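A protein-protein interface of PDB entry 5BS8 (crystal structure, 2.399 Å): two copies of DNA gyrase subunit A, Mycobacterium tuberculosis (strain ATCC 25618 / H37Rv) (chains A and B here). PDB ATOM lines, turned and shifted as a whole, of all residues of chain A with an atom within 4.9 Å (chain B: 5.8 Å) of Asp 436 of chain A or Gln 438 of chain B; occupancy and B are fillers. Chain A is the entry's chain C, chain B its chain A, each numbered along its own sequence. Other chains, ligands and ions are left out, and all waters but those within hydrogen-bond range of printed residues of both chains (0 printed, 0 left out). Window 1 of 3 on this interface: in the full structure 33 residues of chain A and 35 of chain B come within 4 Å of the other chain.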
ATOM      1  N   GLN A 432     -11.992   2.323   9.173  1.00  0.00           N
ATOM      2  CA  GLN A 432     -12.091   3.776   9.203  1.00  0.00           C
ATOM      3  C   GLN A 432     -11.694   4.360   7.852  1.00  0.00           C
ATOM      4  O   GLN A 432     -12.250   5.366   7.411  1.00  0.00           O
ATOM      5  CB  GLN A 432     -11.202   4.349  10.309  1.00  0.00           C
ATOM      6  CG  GLN A 432     -11.538   5.775  10.701  1.00  0.00           C
ATOM      7  CD  GLN A 432     -12.875   5.878  11.403  1.00  0.00           C
ATOM      8  OE1 GLN A 432     -13.904   6.126  10.772  1.00  0.00           O
ATOM      9  NE2 GLN A 432     -12.872   5.682  12.717  1.00  0.00           N
ATOM     10  N   ALA A 433     -10.731   3.716   7.198  1.00  0.00           N
ATOM     11  CA  ALA A 433     -10.248   4.168   5.899  1.00  0.00           C
ATOM     12  C   ALA A 433     -11.298   3.934   4.821  1.00  0.00           C
ATOM     13  O   ALA A 433     -11.460   4.748   3.913  1.00  0.00           O
ATOM     14  CB  ALA A 433      -8.953   3.462   5.539  1.00  0.00           C
ATOM     15  N   ILE A 434     -12.004   2.812   4.923  1.00  0.00           N
ATOM     16  CA  ILE A 434     -13.092   2.509   4.002  1.00  0.00           C
ATOM     17  C   ILE A 434     -14.163   3.588   4.116  1.00  0.00           C
ATOM     18  O   ILE A 434     -14.649   4.103   3.110  1.00  0.00           O
ATOM     19  CB  ILE A 434     -13.711   1.120   4.283  1.00  0.00           C
ATOM     20  CG1 ILE A 434     -12.667   0.023   4.067  1.00  0.00           C
ATOM     21  CG2 ILE A 434     -14.925   0.870   3.381  1.00  0.00           C
ATOM     22  CD1 ILE A 434     -13.094  -1.346   4.559  1.00  0.00           C
ATOM     23  N   LEU A 435     -14.514   3.934   5.351  1.00  0.00           N
ATOM     24  CA  LEU A 435     -15.527   4.951   5.605  1.00  0.00           C
ATOM     25  C   LEU A 435     -15.082   6.315   5.083  1.00  0.00           C
ATOM     26  O   LEU A 435     -15.891   7.080   4.556  1.00  0.00           O
ATOM     27  CB  LEU A 435     -15.832   5.033   7.102  1.00  0.00           C
ATOM     28  CG  LEU A 435     -16.737   3.944   7.681  1.00  0.00           C
ATOM     29  CD1 LEU A 435     -16.744   4.011   9.202  1.00  0.00           C
ATOM     30  CD2 LEU A 435     -18.154   4.069   7.140  1.00  0.00           C
ATOM     31  N   ASP A 436     -13.794   6.612   5.226  1.00  0.00           N
ATOM     32  CA  ASP A 436     -13.244   7.890   4.782  1.00  0.00           C
ATOM     33  C   ASP A 436     -13.016   7.918   3.275  1.00  0.00           C
ATOM     34  O   ASP A 436     -12.642   8.949   2.716  1.00  0.00           O
ATOM     35  CB  ASP A 436     -11.925   8.185   5.502  1.00  0.00           C
ATOM     36  CG  ASP A 436     -12.110   8.425   6.988  1.00  0.00           C
ATOM     37  OD1 ASP A 436     -13.191   8.904   7.387  1.00  0.00           O
ATOM     38  OD2 ASP A 436     -11.169   8.136   7.757  1.00  0.00           O
ATOM     39  N   MET A 437     -13.236   6.783   2.620  1.00  0.00           N
ATOM     40  CA  MET A 437     -13.026   6.682   1.182  1.00  0.00           C
ATOM     41  C   MET A 437     -14.000   7.585   0.427  1.00  0.00           C
ATOM     42  O   MET A 437     -15.182   7.654   0.765  1.00  0.00           O
ATOM     43  CB  MET A 437     -13.188   5.231   0.729  1.00  0.00           C
ATOM     44  CG  MET A 437     -12.525   4.917  -0.598  1.00  0.00           C
ATOM     45  SD  MET A 437     -13.056   3.339  -1.292  1.00  0.00           S
ATOM     46  CE  MET A 437     -12.736   2.229   0.076  1.00  0.00           C
ATOM     47  N   GLN A 438     -13.497   8.284  -0.586  1.00  0.00           N
ATOM     48  CA  GLN A 438     -14.335   9.150  -1.412  1.00  0.00           C
ATOM     49  C   GLN A 438     -15.031   8.356  -2.509  1.00  0.00           C
ATOM     50  O   GLN A 438     -14.557   7.294  -2.913  1.00  0.00           O
ATOM     51  CB  GLN A 438     -13.502  10.267  -2.039  1.00  0.00           C
ATOM     52  CG  GLN A 438     -13.042  11.321  -1.055  1.00  0.00           C
ATOM     53  CD  GLN A 438     -12.179  12.382  -1.706  1.00  0.00           C
ATOM     54  OE1 GLN A 438     -11.176  12.073  -2.350  1.00  0.00           O
ATOM     55  NE2 GLN A 438     -12.570  13.640  -1.550  1.00  0.00           N
ATOM     56  N   ILE B 434     -20.167  16.147  -4.973  1.00  0.00           N
ATOM     57  CA  ILE B 434     -20.673  14.786  -4.840  1.00  0.00           C
ATOM     58  C   ILE B 434     -19.504  13.812  -4.933  1.00  0.00           C
ATOM     59  O   ILE B 434     -19.413  12.861  -4.161  1.00  0.00           O
ATOM     60  CB  ILE B 434     -21.723  14.457  -5.927  1.00  0.00           C
ATOM     61  CG1 ILE B 434     -22.964  15.332  -5.748  1.00  0.00           C
ATOM     62  CG2 ILE B 434     -22.132  12.984  -5.874  1.00  0.00           C
ATOM     63  CD1 ILE B 434     -23.858  15.384  -6.965  1.00  0.00           C
ATOM     64  N   ASP B 436     -16.367  14.293  -4.211  1.00  0.00           N
ATOM     65  CA  ASP B 436     -15.496  14.382  -3.044  1.00  0.00           C
ATOM     66  C   ASP B 436     -16.165  13.834  -1.783  1.00  0.00           C
ATOM     67  O   ASP B 436     -15.544  13.774  -0.721  1.00  0.00           O
ATOM     68  CB  ASP B 436     -15.070  15.835  -2.814  1.00  0.00           C
ATOM     69  CG  ASP B 436     -14.281  16.406  -3.977  1.00  0.00           C
ATOM     70  OD1 ASP B 436     -13.566  15.634  -4.654  1.00  0.00           O
ATOM     71  OD2 ASP B 436     -14.373  17.630  -4.212  1.00  0.00           O
ATOM     72  N   MET B 437     -17.426  13.435  -1.902  1.00  0.00           N
ATOM     73  CA  MET B 437     -18.188  12.944  -0.760  1.00  0.00           C
ATOM     74  C   MET B 437     -17.628  11.622  -0.237  1.00  0.00           C
ATOM     75  O   MET B 437     -17.262  10.742  -1.016  1.00  0.00           O
ATOM     76  CB  MET B 437     -19.654  12.772  -1.147  1.00  0.00           C
ATOM     77  CG  MET B 437     -20.616  12.757   0.023  1.00  0.00           C
ATOM     78  SD  MET B 437     -22.244  12.133  -0.437  1.00  0.00           S
ATOM     79  CE  MET B 437     -22.492  12.912  -2.037  1.00  0.00           C
ATOM     80  N   GLN B 438     -17.561  11.492   1.086  1.00  0.00           N
ATOM     81  CA  GLN B 438     -17.079  10.268   1.721  1.00  0.00           C
ATOM     82  C   GLN B 438     -18.226   9.298   1.972  1.00  0.00           C
ATOM     83  O   GLN B 438     -19.376   9.712   2.115  1.00  0.00           O
ATOM     84  CB  GLN B 438     -16.378  10.591   3.041  1.00  0.00           C
ATOM     85  CG  GLN B 438     -15.077  11.352   2.879  1.00  0.00           C
ATOM     86  CD  GLN B 438     -14.488  11.773   4.206  1.00  0.00           C
ATOM     87  OE1 GLN B 438     -15.152  12.427   5.011  1.00  0.00           O
ATOM     88  NE2 GLN B 438     -13.239  11.391   4.451  1.00  0.00           N
ATOM     89  N   LEU B 439     -17.909   8.008   2.028  1.00  0.00           N
ATOM     90  CA  LEU B 439     -18.917   6.991   2.301  1.00  0.00           C
ATOM     91  C   LEU B 439     -19.501   7.171   3.698  1.00  0.00           C
ATOM     92  O   LEU B 439     -20.600   6.694   3.981  1.00  0.00           O
ATOM     93  CB  LEU B 439     -18.326   5.586   2.160  1.00  0.00           C
ATOM     94  CG  LEU B 439     -17.739   5.209   0.798  1.00  0.00           C
ATOM     95  CD1 LEU B 439     -17.246   3.773   0.822  1.00  0.00           C
ATOM     96  CD2 LEU B 439     -18.749   5.400  -0.319  1.00  0.00           C
ATOM     97  N   ARG B 440     -18.756   7.853   4.565  1.00  0.00           N
ATOM     98  CA  ARG B 440     -19.228   8.185   5.906  1.00  0.00           C
ATOM     99  C   ARG B 440     -20.633   8.775   5.891  1.00  0.00           C
ATOM    100  O   ARG B 440     -21.475   8.421   6.718  1.00  0.00           O
ATOM    101  CB  ARG B 440     -18.279   9.178   6.573  1.00  0.00           C
ATOM    102  CG  ARG B 440     -17.174   8.545   7.383  1.00  0.00           C
ATOM    103  CD  ARG B 440     -16.279   9.610   7.985  1.00  0.00           C
ATOM    104  NE  ARG B 440     -15.311   9.058   8.931  1.00  0.00           N
ATOM    105  CZ  ARG B 440     -15.564   8.815  10.213  1.00  0.00           C
ATOM    106  NH1 ARG B 440     -16.764   9.063  10.723  1.00  0.00           N
ATOM    107  NH2 ARG B 440     -14.613   8.316  10.990  1.00  0.00           N
ATOM    108  N   ARG B 441     -20.877   9.673   4.942  1.00  0.00           N
ATOM    109  CA  ARG B 441     -22.119  10.435   4.908  1.00  0.00           C
ATOM    110  C   ARG B 441     -23.278   9.678   4.256  1.00  0.00           C
ATOM    111  O   ARG B 441     -24.358  10.237   4.068  1.00  0.00           O
ATOM    112  CB  ARG B 441     -21.893  11.766   4.185  1.00  0.00           C
ATOM    113  CG  ARG B 441     -21.194  12.810   5.046  1.00  0.00           C
ATOM    114  CD  ARG B 441     -21.147  14.170   4.371  1.00  0.00           C
ATOM    115  NE  ARG B 441     -20.038  14.284   3.429  1.00  0.00           N
ATOM    116  CZ  ARG B 441     -19.689  15.413   2.820  1.00  0.00           C
ATOM    117  NH1 ARG B 441     -20.362  16.532   3.050  1.00  0.00           N
ATOM    118  NH2 ARG B 441     -18.661  15.424   1.981  1.00  0.00           N
ATOM    119  N   LEU B 442     -23.054   8.409   3.921  1.00  0.00           N
ATOM    120  CA  LEU B 442     -24.108   7.571   3.353  1.00  0.00           C
ATOM    121  C   LEU B 442     -24.898   6.839   4.442  1.00  0.00           C
ATOM    122  O   LEU B 442     -25.883   6.157   4.152  1.00  0.00           O
ATOM    123  CB  LEU B 442     -23.516   6.562   2.365  1.00  0.00           C
ATOM    124  CG  LEU B 442     -22.852   7.149   1.115  1.00  0.00           C
ATOM    125  CD1 LEU B 442     -22.369   6.032   0.201  1.00  0.00           C
ATOM    126  CD2 LEU B 442     -23.795   8.080   0.358  1.00  0.00           C
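The backbone NH of Leu 439 of chain B is in hydrogen-bond range of the backbone carbonyl oxygen of Met 437 of chain A (3.0 Å). The side-chain amide oxygen of Gln 432 of chain A lies close to the guanidinium group of Arg 440 of chain B (2.3 Å). The backbone carbonyl oxygen of Asp 436 of chain B sits at hydrogen-bond distance from the side-chain amide nitrogen of Gln 438 of chain A. N of Arg 440 of chain B is in hydrogen-bond range of O of Leu 435 of chain A (3.0 Å). The guanidinium group (NE) of Arg 440 of chain B lies within salt-bridge range of the side-chain carboxylate (OD1) of Asp 436 of chain A (2.6 Å). NE2 of Gln 438 of chain B sits at hydrogen-bond distance from O of Asp 436 of chain A (3.1 Å). O of Leu 435 of chain A lies within hydrogen-bond range of N of Leu 439 of chain B.
Among the printed residues, pairs that only touch across the chains: Gln 438 of chain A with Met 437 of chain B (3.4 Å), Met 437 of chain A with Gln 438 of chain B (3.4 Å), Ile 434 of chain A with Leu 439 of chain B (3.5 Å) and Leu 435 of chain A with Gln 438 of chain B (3.9 Å).
Ala 433 of chain A touches none of the printed residues of chain B. Of chain B, only Gln 438 and Arg 440 come within 4 Å of Asp 436 of chain A. Printed residues of chain B within 4 Å of Gln 438 of chain A: Asp 436 and Met 437. Ile 434 of chain B touches none of the printed residues of chain A. Gln 438 of chain B touches just these residues of chain A: Leu 435 (3.9 Å), Asp 436 (3.1 Å) and Met 437 (3.4 Å). Of the printed residues of chain A, Arg 440 of chain B touches Gln 432 (2.3 Å), Leu 435 (3.0 Å) and Asp 436 (2.6 Å). The nearest residue of chain A that does not touch Gln 438 of chain B is Gln 438 of chain A (4.3 Å). The nearest printed residue of chain A that does not touch Leu 439 of chain B is Asp 436 of chain A (5.1 Å).
Hydrophobic or aromatic side chains of chain B that line the printed part of chain A: Leu 439. Hydrophobic or aromatic side chains of chain A within 4 Å of the printed part of chain B: Leu 435.
Asp 436 of chain A touches Gln 438 of chain B, and with the chains exchanged Gln 438 of chain A touches Asp 436 of chain B. Met 437 of chain A touches Gln 438 of chain B, and with the chains exchanged Gln 438 of chain A touches Met 437 of chain B. 4 positions are printed for both chains. Of the 11 pairs that touch across the chains among the printed residues, 4 have their exchanged pair printed and touching as well.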
